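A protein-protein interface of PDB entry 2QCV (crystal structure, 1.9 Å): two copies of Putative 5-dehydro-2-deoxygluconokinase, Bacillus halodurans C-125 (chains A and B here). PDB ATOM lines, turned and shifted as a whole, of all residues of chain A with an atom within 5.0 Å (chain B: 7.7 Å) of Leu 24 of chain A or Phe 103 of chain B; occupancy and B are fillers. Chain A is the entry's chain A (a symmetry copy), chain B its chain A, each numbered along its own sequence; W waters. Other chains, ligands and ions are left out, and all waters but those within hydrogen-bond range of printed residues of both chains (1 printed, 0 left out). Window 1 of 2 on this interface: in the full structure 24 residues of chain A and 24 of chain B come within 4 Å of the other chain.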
ATOM      1  N   ILE A  22     -24.382   3.185  28.660  1.00  0.00           N
ATOM      2  CA  ILE A  22     -25.017   4.505  28.645  1.00  0.00           C
ATOM      3  C   ILE A  22     -25.632   4.769  27.288  1.00  0.00           C
ATOM      4  O   ILE A  22     -24.970   4.669  26.250  1.00  0.00           O
ATOM      5  CB  ILE A  22     -24.001   5.604  28.947  1.00  0.00           C
ATOM      6  CG1 ILE A  22     -23.403   5.386  30.355  1.00  0.00           C
ATOM      7  CG2 ILE A  22     -24.657   7.050  28.841  1.00  0.00           C
ATOM      8  CD1 ILE A  22     -24.456   5.503  31.449  1.00  0.00           C
ATOM      9  N   ASP A  23     -26.897   5.154  27.312  1.00  0.00           N
ATOM     10  CA  ASP A  23     -27.555   5.715  26.143  1.00  0.00           C
ATOM     11  C   ASP A  23     -27.624   7.240  26.329  1.00  0.00           C
ATOM     12  O   ASP A  23     -27.958   7.754  27.411  1.00  0.00           O
ATOM     13  CB  ASP A  23     -28.962   5.171  25.991  1.00  0.00           C
ATOM     14  CG  ASP A  23     -29.006   3.751  25.431  1.00  0.00           C
ATOM     15  OD1 ASP A  23     -27.954   3.160  25.116  1.00  0.00           O
ATOM     16  OD2 ASP A  23     -30.130   3.243  25.326  1.00  0.00           O
ATOM     17  N   LEU A  24     -27.284   7.947  25.266  1.00  0.00           N
ATOM     18  CA  LEU A  24     -27.350   9.403  25.221  1.00  0.00           C
ATOM     19  C   LEU A  24     -28.372   9.726  24.134  1.00  0.00           C
ATOM     20  O   LEU A  24     -28.102   9.658  22.945  1.00  0.00           O
ATOM     21  CB  LEU A  24     -25.969   9.984  24.972  1.00  0.00           C
ATOM     22  CG  LEU A  24     -25.047   9.813  26.210  1.00  0.00           C
ATOM     23  CD1 LEU A  24     -23.563   9.843  25.890  1.00  0.00           C
ATOM     24  CD2 LEU A  24     -25.391  10.838  27.243  1.00  0.00           C
ATOM     25  N   ASN A  25     -29.564  10.048  24.599  1.00  0.00           N
ATOM     26  CA  ASN A  25     -30.692  10.301  23.756  1.00  0.00           C
ATOM     27  C   ASN A  25     -30.866  11.766  23.395  1.00  0.00           C
ATOM     28  O   ASN A  25     -30.910  12.621  24.250  1.00  0.00           O
ATOM     29  CB  ASN A  25     -31.946   9.813  24.463  1.00  0.00           C
ATOM     30  CG  ASN A  25     -31.914   8.315  24.681  1.00  0.00           C
ATOM     31  OD1 ASN A  25     -31.976   7.849  25.815  1.00  0.00           O
ATOM     32  ND2 ASN A  25     -31.746   7.556  23.595  1.00  0.00           N
ATOM     33  N   ALA A  26     -30.966  12.000  22.101  1.00  0.00           N
ATOM     34  CA  ALA A  26     -31.126  13.308  21.513  1.00  0.00           C
ATOM     35  C   ALA A  26     -32.344  13.996  22.062  1.00  0.00           C
ATOM     36  O   ALA A  26     -33.459  13.467  21.938  1.00  0.00           O
ATOM     37  CB  ALA A  26     -31.283  13.144  19.996  1.00  0.00           C
ATOM     38  N   PHE A  39     -28.257  15.998  24.998  1.00  0.00           N
ATOM     39  CA  PHE A  39     -28.496  14.554  25.104  1.00  0.00           C
ATOM     40  C   PHE A  39     -28.857  14.217  26.535  1.00  0.00           C
ATOM     41  O   PHE A  39     -28.237  14.757  27.464  1.00  0.00           O
ATOM     42  CB  PHE A  39     -27.237  13.758  24.721  1.00  0.00           C
ATOM     43  CG  PHE A  39     -26.851  13.899  23.278  1.00  0.00           C
ATOM     44  CD1 PHE A  39     -27.375  13.055  22.313  1.00  0.00           C
ATOM     45  CD2 PHE A  39     -25.971  14.887  22.891  1.00  0.00           C
ATOM     46  CE1 PHE A  39     -27.022  13.186  20.979  1.00  0.00           C
ATOM     47  CE2 PHE A  39     -25.619  15.038  21.559  1.00  0.00           C
ATOM     48  CZ  PHE A  39     -26.148  14.192  20.598  1.00  0.00           C
ATOM     49  N   SER A  40     -29.854  13.346  26.708  1.00  0.00           N
ATOM     50  CA  SER A  40     -30.219  12.864  28.038  1.00  0.00           C
ATOM     51  C   SER A  40     -29.616  11.478  28.292  1.00  0.00           C
ATOM     52  O   SER A  40     -29.605  10.614  27.404  1.00  0.00           O
ATOM     53  CB  SER A  40     -31.739  12.844  28.205  1.00  0.00           C
ATOM     54  OG  SER A  40     -32.324  12.131  27.142  1.00  0.00           O
ATOM     55  N   LYS A  41     -29.090  11.306  29.500  1.00  0.00           N
ATOM     56  CA  LYS A  41     -28.386  10.102  29.937  1.00  0.00           C
ATOM     57  C   LYS A  41     -29.337   9.057  30.519  1.00  0.00           C
ATOM     58  O   LYS A  41     -30.067   9.324  31.484  1.00  0.00           O
ATOM     59  CB  LYS A  41     -27.379  10.479  31.013  1.00  0.00           C
ATOM     60  CG  LYS A  41     -26.436   9.401  31.424  1.00  0.00           C
ATOM     61  CD  LYS A  41     -25.508   9.845  32.520  1.00  0.00           C
ATOM     62  CE  LYS A  41     -26.237   9.975  33.845  1.00  0.00           C
ATOM     63  NZ  LYS A  41     -25.345  10.402  34.944  1.00  0.00           N
ATOM     64  N   HIS A  72     -19.910   6.785  35.033  1.00  0.00           N
ATOM     65  CA  HIS A  72     -20.910   6.115  34.232  1.00  0.00           C
ATOM     66  C   HIS A  72     -21.254   4.722  34.822  1.00  0.00           C
ATOM     67  O   HIS A  72     -22.421   4.369  34.939  1.00  0.00           O
ATOM     68  CB  HIS A  72     -20.445   6.002  32.782  1.00  0.00           C
ATOM     69  CG  HIS A  72     -20.520   7.285  32.020  1.00  0.00           C
ATOM     70  ND1 HIS A  72     -21.317   8.339  32.405  1.00  0.00           N
ATOM     71  CD2 HIS A  72     -19.949   7.655  30.848  1.00  0.00           C
ATOM     72  CE1 HIS A  72     -21.186   9.328  31.538  1.00  0.00           C
ATOM     73  NE2 HIS A  72     -20.380   8.930  30.571  1.00  0.00           N
ATOM     74  N   LEU A 101     -21.151   3.436  24.826  1.00  0.00           N
ATOM     75  CA  LEU A 101     -22.015   4.617  24.680  1.00  0.00           C
ATOM     76  C   LEU A 101     -22.809   4.486  23.401  1.00  0.00           C
ATOM     77  O   LEU A 101     -22.261   4.130  22.341  1.00  0.00           O
ATOM     78  CB  LEU A 101     -21.199   5.920  24.560  1.00  0.00           C
ATOM     79  CG  LEU A 101     -20.265   6.310  25.701  1.00  0.00           C
ATOM     80  CD1 LEU A 101     -19.420   7.564  25.347  1.00  0.00           C
ATOM     81  CD2 LEU A 101     -21.064   6.531  26.971  1.00  0.00           C
ATOM     82  N   ALA A 102     -24.094   4.784  23.488  1.00  0.00           N
ATOM     83  CA  ALA A 102     -24.932   4.832  22.294  1.00  0.00           C
ATOM     84  C   ALA A 102     -25.515   6.237  22.188  1.00  0.00           C
ATOM     85  O   ALA A 102     -26.325   6.615  23.010  1.00  0.00           O
ATOM     86  CB  ALA A 102     -26.039   3.776  22.396  1.00  0.00           C
ATOM     87  N   PHE A 103     -25.098   7.009  21.187  1.00  0.00           N
ATOM     88  CA  PHE A 103     -25.739   8.290  20.896  1.00  0.00           C
ATOM     89  C   PHE A 103     -26.836   8.042  19.885  1.00  0.00           C
ATOM     90  O   PHE A 103     -26.596   7.419  18.836  1.00  0.00           O
ATOM     91  CB  PHE A 103     -24.757   9.273  20.278  1.00  0.00           C
ATOM     92  CG  PHE A 103     -23.671   9.728  21.199  1.00  0.00           C
ATOM     93  CD1 PHE A 103     -22.531   8.951  21.389  1.00  0.00           C
ATOM     94  CD2 PHE A 103     -23.765  10.967  21.831  1.00  0.00           C
ATOM     95  CE1 PHE A 103     -21.524   9.398  22.244  1.00  0.00           C
ATOM     96  CE2 PHE A 103     -22.748  11.421  22.657  1.00  0.00           C
ATOM     97  CZ  PHE A 103     -21.661  10.644  22.880  1.00  0.00           C
ATOM     98  N   THR A 104     -28.030   8.533  20.161  1.00  0.00           N
ATOM     99  CA  THR A 104     -29.161   8.185  19.279  1.00  0.00           C
ATOM    100  C   THR A 104     -29.465   9.338  18.365  1.00  0.00           C
ATOM    101  O   THR A 104     -29.410  10.501  18.778  1.00  0.00           O
ATOM    102  CB  THR A 104     -30.415   7.825  20.077  1.00  0.00           C
ATOM    103  OG1 THR A 104     -30.795   8.974  20.844  1.00  0.00           O
ATOM    104  CG2 THR A 104     -30.138   6.637  20.973  1.00  0.00           C
ATOM    105  N   ILE B  22     -15.328  16.186  20.898  1.00  0.00           N
ATOM    106  CA  ILE B  22     -16.613  16.553  21.497  1.00  0.00           C
ATOM    107  C   ILE B  22     -16.463  16.697  22.996  1.00  0.00           C
ATOM    108  O   ILE B  22     -15.981  15.793  23.686  1.00  0.00           O
ATOM    109  CB  ILE B  22     -17.673  15.492  21.209  1.00  0.00           C
ATOM    110  CG1 ILE B  22     -17.884  15.370  19.684  1.00  0.00           C
ATOM    111  CG2 ILE B  22     -19.049  15.830  21.934  1.00  0.00           C
ATOM    112  CD1 ILE B  22     -18.428  16.656  19.076  1.00  0.00           C
ATOM    113  N   ASP B  23     -16.926  17.830  23.499  1.00  0.00           N
ATOM    114  CA  ASP B  23     -17.121  18.018  24.927  1.00  0.00           C
ATOM    115  C   ASP B  23     -18.623  17.873  25.220  1.00  0.00           C
ATOM    116  O   ASP B  23     -19.486  18.409  24.502  1.00  0.00           O
ATOM    117  CB  ASP B  23     -16.661  19.393  25.368  1.00  0.00           C
ATOM    118  CG  ASP B  23     -15.143  19.519  25.479  1.00  0.00           C
ATOM    119  OD1 ASP B  23     -14.406  18.540  25.249  1.00  0.00           O
ATOM    120  OD2 ASP B  23     -14.713  20.635  25.795  1.00  0.00           O
ATOM    121  N   LEU B  24     -18.918  17.125  26.269  1.00  0.00           N
ATOM    122  CA  LEU B  24     -20.280  16.924  26.749  1.00  0.00           C
ATOM    123  C   LEU B  24     -20.304  17.520  28.154  1.00  0.00           C
ATOM    124  O   LEU B  24     -19.831  16.935  29.117  1.00  0.00           O
ATOM    125  CB  LEU B  24     -20.645  15.451  26.688  1.00  0.00           C
ATOM    126  CG  LEU B  24     -20.821  14.967  25.223  1.00  0.00           C
ATOM    127  CD1 LEU B  24     -20.636  13.471  25.035  1.00  0.00           C
ATOM    128  CD2 LEU B  24     -22.149  15.411  24.700  1.00  0.00           C
ATOM    129  N   ASN B  25     -20.846  18.721  28.217  1.00  0.00           N
ATOM    130  CA  ASN B  25     -20.892  19.498  29.417  1.00  0.00           C
ATOM    131  C   ASN B  25     -22.167  19.305  30.220  1.00  0.00           C
ATOM    132  O   ASN B  25     -23.255  19.445  29.709  1.00  0.00           O
ATOM    133  CB  ASN B  25     -20.754  20.967  29.050  1.00  0.00           C
ATOM    134  CG  ASN B  25     -19.411  21.258  28.414  1.00  0.00           C
ATOM    135  OD1 ASN B  25     -19.347  21.721  27.279  1.00  0.00           O
ATOM    136  ND2 ASN B  25     -18.329  20.918  29.119  1.00  0.00           N
ATOM    137  N   ALA B  26     -21.971  18.989  31.485  1.00  0.00           N
ATOM    138  CA  ALA B  26     -23.024  18.745  32.443  1.00  0.00           C
ATOM    139  C   ALA B  26     -23.940  19.932  32.543  1.00  0.00           C
ATOM    140  O   ALA B  26     -23.483  21.038  32.868  1.00  0.00           O
ATOM    141  CB  ALA B  26     -22.385  18.486  33.813  1.00  0.00           C
ATOM    142  N   MET B  33     -21.203  13.583  38.633  1.00  0.00           N
ATOM    143  CA  MET B  33     -21.705  13.329  37.298  1.00  0.00           C
ATOM    144  C   MET B  33     -22.761  12.219  37.295  1.00  0.00           C
ATOM    145  O   MET B  33     -23.630  12.206  36.433  1.00  0.00           O
ATOM    146  CB  MET B  33     -20.556  12.956  36.348  1.00  0.00           C
ATOM    147  CG  MET B  33     -21.021  12.578  34.952  1.00  0.00           C
ATOM    148  SD  MET B  33     -19.562  11.885  33.869  1.00  0.00           S
ATOM    149  CE  MET B  33     -18.455  13.393  34.097  1.00  0.00           C
ATOM    150  N   THR B  36     -25.864  13.914  37.107  1.00  0.00           N
ATOM    151  CA  THR B  36     -26.052  14.780  35.947  1.00  0.00           C
ATOM    152  C   THR B  36     -26.765  13.979  34.903  1.00  0.00           C
ATOM    153  O   THR B  36     -26.216  12.986  34.417  1.00  0.00           O
ATOM    154  CB  THR B  36     -24.713  15.240  35.348  1.00  0.00           C
ATOM    155  OG1 THR B  36     -24.052  16.110  36.265  1.00  0.00           O
ATOM    156  CG2 THR B  36     -24.917  15.951  34.001  1.00  0.00           C
ATOM    157  N   MET B  37     -27.967  14.424  34.543  1.00  0.00           N
ATOM    158  CA  MET B  37     -28.843  13.713  33.648  1.00  0.00           C
ATOM    159  C   MET B  37     -28.833  14.230  32.222  1.00  0.00           C
ATOM    160  O   MET B  37     -29.317  13.535  31.334  1.00  0.00           O
ATOM    161  CB  MET B  37     -30.263  13.773  34.181  1.00  0.00           C
ATOM    162  CG  MET B  37     -30.417  13.110  35.567  1.00  0.00           C
ATOM    163  SD  MET B  37     -29.581  11.303  35.722  1.00  0.00           S
ATOM    164  CE  MET B  37     -30.650  10.315  34.472  1.00  0.00           C
ATOM    165  N   THR B  38     -28.333  15.450  32.011  1.00  0.00           N
ATOM    166  CA  THR B  38     -28.300  16.047  30.667  1.00  0.00           C
ATOM    167  C   THR B  38     -26.950  16.710  30.383  1.00  0.00           C
ATOM    168  O   THR B  38     -26.345  17.291  31.267  1.00  0.00           O
ATOM    169  CB  THR B  38     -29.447  17.078  30.510  1.00  0.00           C
ATOM    170  OG1 THR B  38     -30.639  16.522  31.083  1.00  0.00           O
ATOM    171  CG2 THR B  38     -29.714  17.365  29.058  1.00  0.00           C
ATOM    172  N   PHE B  39     -26.488  16.577  29.138  1.00  0.00           N
ATOM    173  CA  PHE B  39     -25.179  17.082  28.707  1.00  0.00           C
ATOM    174  C   PHE B  39     -25.356  17.891  27.440  1.00  0.00           C
ATOM    175  O   PHE B  39     -26.122  17.480  26.555  1.00  0.00           O
ATOM    176  CB  PHE B  39     -24.212  15.923  28.412  1.00  0.00           C
ATOM    177  CG  PHE B  39     -23.845  15.121  29.625  1.00  0.00           C
ATOM    178  CD1 PHE B  39     -22.773  15.483  30.424  1.00  0.00           C
ATOM    179  CD2 PHE B  39     -24.586  14.010  29.970  1.00  0.00           C
ATOM    180  CE1 PHE B  39     -22.435  14.745  31.547  1.00  0.00           C
ATOM    181  CE2 PHE B  39     -24.267  13.270  31.098  1.00  0.00           C
ATOM    182  CZ  PHE B  39     -23.194  13.639  31.894  1.00  0.00           C
ATOM    183  N   HIS B  72     -20.476  13.180  14.731  1.00  0.00           N
ATOM    184  CA  HIS B  72     -19.655  14.008  15.587  1.00  0.00           C
ATOM    185  C   HIS B  72     -18.560  14.742  14.768  1.00  0.00           C
ATOM    186  O   HIS B  72     -18.352  15.936  14.943  1.00  0.00           O
ATOM    187  CB  HIS B  72     -19.041  13.173  16.708  1.00  0.00           C
ATOM    188  CG  HIS B  72     -20.007  12.804  17.787  1.00  0.00           C
ATOM    189  ND1 HIS B  72     -21.184  13.484  18.003  1.00  0.00           N
ATOM    190  CD2 HIS B  72     -19.930  11.866  18.762  1.00  0.00           C
ATOM    191  CE1 HIS B  72     -21.823  12.941  19.025  1.00  0.00           C
ATOM    192  NE2 HIS B  72     -21.074  11.973  19.518  1.00  0.00           N
ATOM    193  N   GLY B 100     -12.799  11.598  19.997  1.00  0.00           N
ATOM    194  CA  GLY B 100     -12.652  11.615  21.456  1.00  0.00           C
ATOM    195  C   GLY B 100     -13.781  12.366  22.127  1.00  0.00           C
ATOM    196  O   GLY B 100     -14.402  13.252  21.523  1.00  0.00           O
ATOM    197  N   LEU B 101     -14.075  11.999  23.367  1.00  0.00           N
ATOM    198  CA  LEU B 101     -15.204  12.567  24.120  1.00  0.00           C
ATOM    199  C   LEU B 101     -14.721  12.970  25.493  1.00  0.00           C
ATOM    200  O   LEU B 101     -13.999  12.211  26.167  1.00  0.00           O
ATOM    201  CB  LEU B 101     -16.333  11.539  24.336  1.00  0.00           C
ATOM    202  CG  LEU B 101     -17.005  10.919  23.114  1.00  0.00           C
ATOM    203  CD1 LEU B 101     -18.010   9.805  23.517  1.00  0.00           C
ATOM    204  CD2 LEU B 101     -17.687  11.998  22.295  1.00  0.00           C
ATOM    205  N   ALA B 102     -15.123  14.155  25.920  1.00  0.00           N
ATOM    206  CA  ALA B 102     -14.840  14.594  27.284  1.00  0.00           C
ATOM    207  C   ALA B 102     -16.172  14.870  27.972  1.00  0.00           C
ATOM    208  O   ALA B 102     -16.856  15.805  27.605  1.00  0.00           O
ATOM    209  CB  ALA B 102     -13.959  15.848  27.250  1.00  0.00           C
ATOM    210  N   PHE B 103     -16.542  14.057  28.959  1.00  0.00           N
ATOM    211  CA  PHE B 103     -17.700  14.357  29.797  1.00  0.00           C
ATOM    212  C   PHE B 103     -17.216  15.144  30.996  1.00  0.00           C
ATOM    213  O   PHE B 103     -16.270  14.724  31.683  1.00  0.00           O
ATOM    214  CB  PHE B 103     -18.353  13.085  30.316  1.00  0.00           C
ATOM    215  CG  PHE B 103     -19.003  12.247  29.262  1.00  0.00           C
ATOM    216  CD1 PHE B 103     -18.250  11.361  28.496  1.00  0.00           C
ATOM    217  CD2 PHE B 103     -20.384  12.304  29.079  1.00  0.00           C
ATOM    218  CE1 PHE B 103     -18.878  10.581  27.525  1.00  0.00           C
ATOM    219  CE2 PHE B 103     -21.008  11.504  28.133  1.00  0.00           C
ATOM    220  CZ  PHE B 103     -20.269  10.677  27.354  1.00  0.00           C
ATOM    221  N   THR B 104     -17.857  16.263  31.278  1.00  0.00           N
ATOM    222  CA  THR B 104     -17.322  17.135  32.342  1.00  0.00           C
ATOM    223  C   THR B 104     -18.133  16.961  33.595  1.00  0.00           C
ATOM    224  O   THR B 104     -19.360  16.827  33.539  1.00  0.00           O
ATOM    225  CB  THR B 104     -17.336  18.608  31.930  1.00  0.00           C
ATOM    226  OG1 THR B 104     -18.697  18.988  31.693  1.00  0.00           O
ATOM    227  CG2 THR B 104     -16.489  18.810  30.691  1.00  0.00           C
ATOM    228  N   GLU B 105     -17.427  16.852  34.722  1.00  0.00           N
ATOM    229  CA  GLU B 105     -18.054  16.808  36.031  1.00  0.00           C
ATOM    230  C   GLU B 105     -17.669  18.087  36.739  1.00  0.00           C
ATOM    231  O   GLU B 105     -16.489  18.433  36.765  1.00  0.00           O
ATOM    232  CB  GLU B 105     -17.531  15.636  36.859  1.00  0.00           C
ATOM    233  CG  GLU B 105     -18.119  15.601  38.248  1.00  0.00           C
ATOM    234  CD  GLU B 105     -17.646  14.411  39.038  1.00  0.00           C
ATOM    235  OE1 GLU B 105     -16.514  14.476  39.573  1.00  0.00           O
ATOM    236  OE2 GLU B 105     -18.391  13.405  39.085  1.00  0.00           O
ATOM    237  N   ILE B 106     -18.664  18.761  37.306  1.00  0.00           N
ATOM    238  CA  ILE B 106     -18.474  19.949  38.136  1.00  0.00           C
ATOM    239  C   ILE B 106     -19.093  19.667  39.502  1.00  0.00           C
ATOM    240  O   ILE B 106     -20.300  19.820  39.704  1.00  0.00           O
ATOM    241  CB  ILE B 106     -19.135  21.194  37.483  1.00  0.00           C
ATOM    242  CG1 ILE B 106     -18.673  21.334  36.021  1.00  0.00           C
ATOM    243  CG2 ILE B 106     -18.755  22.485  38.225  1.00  0.00           C
ATOM    244  CD1 ILE B 106     -19.588  22.184  35.188  1.00  0.00           C
ATOM    245  N   SER B 113     -13.590  17.903  36.712  1.00  0.00           N
ATOM    246  CA  SER B 113     -12.777  16.839  36.117  1.00  0.00           C
ATOM    247  C   SER B 113     -13.486  16.311  34.874  1.00  0.00           C
ATOM    248  O   SER B 113     -14.660  16.610  34.654  1.00  0.00           O
ATOM    249  CB  SER B 113     -12.575  15.705  37.111  1.00  0.00           C
ATOM    250  OG  SER B 113     -13.812  15.155  37.506  1.00  0.00           O
ATOM    251  N   ILE B 114     -12.769  15.524  34.085  1.00  0.00           N
ATOM    252  CA  ILE B 114     -13.284  15.030  32.828  1.00  0.00           C
ATOM    253  C   ILE B 114     -13.206  13.499  32.856  1.00  0.00           C
ATOM    254  O   ILE B 114     -12.182  12.923  33.282  1.00  0.00           O
ATOM    255  CB  ILE B 114     -12.498  15.636  31.632  1.00  0.00           C
ATOM    256  CG1 ILE B 114     -12.959  17.070  31.364  1.00  0.00           C
ATOM    257  CG2 ILE B 114     -12.640  14.813  30.368  1.00  0.00           C
ATOM    258  CD1 ILE B 114     -12.006  17.866  30.471  1.00  0.00           C
ATOM    259  N   LEU B 115     -14.287  12.850  32.427  1.00  0.00           N
ATOM    260  CA  LEU B 115     -14.251  11.428  32.100  1.00  0.00           C
ATOM    261  C   LEU B 115     -13.976  11.388  30.589  1.00  0.00           C
ATOM    262  O   LEU B 115     -14.804  11.849  29.796  1.00  0.00           O
ATOM    263  CB  LEU B 115     -15.597  10.777  32.484  1.00  0.00           C
ATOM    264  CG  LEU B 115     -15.801   9.285  32.178  1.00  0.00           C
ATOM    265  CD1 LEU B 115     -14.582   8.464  32.598  1.00  0.00           C
ATOM    266  CD2 LEU B 115     -17.039   8.797  32.843  1.00  0.00           C
ATOM    267  N   MET B 116     -12.796  10.918  30.198  1.00  0.00           N
ATOM    268  CA  MET B 116     -12.347  10.983  28.820  1.00  0.00           C
ATOM    269  C   MET B 116     -12.431   9.660  28.083  1.00  0.00           C
ATOM    270  O   MET B 116     -12.085   8.610  28.620  1.00  0.00           O
ATOM    271  CB  MET B 116     -10.892  11.480  28.777  1.00  0.00           C
ATOM    272  CG  MET B 116     -10.370  11.762  27.386  1.00  0.00           C
ATOM    273  SD  MET B 116     -10.924  13.560  26.724  1.00  0.00           S
ATOM    274  CE  MET B 116     -10.593  13.310  24.748  1.00  0.00           C
ATOM    275  N   TYR B 117     -12.924   9.714  26.851  1.00  0.00           N
ATOM    276  CA  TYR B 117     -12.859   8.599  25.907  1.00  0.00           C
ATOM    277  C   TYR B 117     -11.743   8.991  24.921  1.00  0.00           C
ATOM    278  O   TYR B 117     -11.927   9.896  24.122  1.00  0.00           O
ATOM    279  CB  TYR B 117     -14.206   8.441  25.202  1.00  0.00           C
ATOM    280  CG  TYR B 117     -15.216   7.738  26.089  1.00  0.00           C
ATOM    281  CD1 TYR B 117     -15.703   8.342  27.249  1.00  0.00           C
ATOM    282  CD2 TYR B 117     -15.650   6.461  25.778  1.00  0.00           C
ATOM    283  CE1 TYR B 117     -16.614   7.681  28.058  1.00  0.00           C
ATOM    284  CE2 TYR B 117     -16.560   5.786  26.582  1.00  0.00           C
ATOM    285  CZ  TYR B 117     -17.034   6.406  27.719  1.00  0.00           C
ATOM    286  OH  TYR B 117     -17.919   5.718  28.513  1.00  0.00           O
ATOM    287  N   PHE B 269     -12.431  24.249  33.052  1.00  0.00           N
ATOM    288  CA  PHE B 269     -12.018  23.738  31.744  1.00  0.00           C
ATOM    289  C   PHE B 269     -11.868  24.901  30.780  1.00  0.00           C
ATOM    290  O   PHE B 269     -12.625  25.865  30.834  1.00  0.00           O
ATOM    291  CB  PHE B 269     -13.065  22.802  31.148  1.00  0.00           C
ATOM    292  CG  PHE B 269     -13.673  21.877  32.137  1.00  0.00           C
ATOM    293  CD1 PHE B 269     -12.914  20.835  32.660  1.00  0.00           C
ATOM    294  CD2 PHE B 269     -14.989  22.068  32.570  1.00  0.00           C
ATOM    295  CE1 PHE B 269     -13.465  19.958  33.581  1.00  0.00           C
ATOM    296  CE2 PHE B 269     -15.557  21.205  33.508  1.00  0.00           C
ATOM    297  CZ  PHE B 269     -14.801  20.141  34.007  1.00  0.00           C
HETATM  298  O   HOH W   1     -31.720  11.379  31.668  1.00  0.00           O
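The backbone carbonyl oxygen (O) of Leu 24 of chain B is in hydrogen-bond range of the backbone NH (N) of Thr 104 of chain B, at 3.0 Å.
O of Leu 101 of chain B lies within hydrogen-bond range of N of Tyr 117 of chain B, 2.8 Å away.
OE2 of Glu 105 of chain B is in hydrogen-bond range of N of Met 33 of chain B.
O of Leu 24 of chain A is in hydrogen-bond range of N of Thr 104 of chain A (3.0 Å).
The backbone carbonyl oxygen (O) of Phe 103 of chain B sits at hydrogen-bond distance from the backbone NH (N) of Leu 115 of chain B, 2.8 Å away.
The backbone NH (N) of Ser 40 of chain A is in hydrogen-bond range of the backbone carbonyl oxygen (O) of Asn 25 of chain A.
Of chain B, only Phe 103 comes within 4 Å of Leu 24 of chain A.
Of chain A, only Leu 24, His 72 and Leu 101 come within 4 Å of Phe 103 of chain B.
Of the printed residues of chain A, Thr 38 of chain B touches Phe 39 (3.4 Å).
Of the printed residues of chain B, Phe 39 of chain A touches Thr 38 (3.4 Å) and Phe 39 (3.0 Å).
Printed residues of chain B within 4 Å of Leu 101 of chain A: Leu 101, Phe 103 and Tyr 117.
The nearest residue of chain B that does not touch Leu 24 of chain A is Phe 39 of chain B (4.3 Å).
The nearest printed residue of chain A that does not touch His 72 of chain B is Phe 39 of chain A (4.8 Å).
Hydrophobic or aromatic side chains of chain B that line the printed part of chain A: Leu 24, Met 33, Met 37, Phe 39, His 72, Leu 101, Phe 103, Leu 115 and Tyr 117.
Of the 13 printed residues of chain A, 7 touch a printed residue of chain B.
Along chain A the printed residues that touch a printed residue of chain B span positions 24 to 103.
Among the printed residues, 18 pairs touch across the chains.
Water W1 bridges the backbone carbonyl oxygen of Lys 41 of chain A (2.6 Å) and the backbone carbonyl oxygen of Met 37 of chain B (3.2 Å).
The side-chain amino group (NZ) of Lys 41 of chain A is in hydrogen-bond range of the backbone carbonyl oxygen (O) of Thr 36 of chain B (2.8 Å).
The backbone carbonyl oxygen (O) of Phe 39 of chain A lies within hydrogen-bond range of the backbone NH (N) of Phe 39 of chain B (3.0 Å).
O of Met 33 of chain B is in hydrogen-bond range of NZ of Lys 41 of chain A, at 2.9 Å.
O of Met 37 of chain B sits at hydrogen-bond distance from N of Lys 41 of chain A.
Leu 24 of chain A touches Phe 103 of chain B, and with the chains exchanged Phe 103 of chain A touches Leu 24 of chain B.
Phe 39 of chain B touches its own counterpart, Phe 39 of chain A.
Leu 101 of chain B touches its own counterpart, Leu 101 of chain A.
Leu 101 of chain A touches Phe 103 of chain B, and with the chains exchanged Phe 103 of chain A touches Leu 101 of chain B.
Of the 18 pairs that touch across the chains among the printed residues, 8 have their exchanged pair printed and touching as well.
Among the printed residues, pairs that only touch across the chains: Leu 24 of chain A with Phe 103 of chain B, Phe 39 of chain A with Thr 38 of chain B, Ser 40 of chain A with Met 37 of chain B, Lys 41 of chain A with Phe 39 of chain B, His 72 of chain A with Met 33 of chain B, His 72 of chain A with Phe 103 of chain B, His 72 of chain A with Leu 115 of chain B, His 72 of chain A with Tyr 117 of chain B, Leu 101 of chain A with Leu 101 of chain B, Leu 101 of chain A with Phe 103 of chain B, Leu 101 of chain A with Tyr 117 of chain B, Phe 103 of chain A with Leu 24 of chain B, Phe 103 of chain A with His 72 of chain B and Phe 103 of chain A with Leu 101 of chain B.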
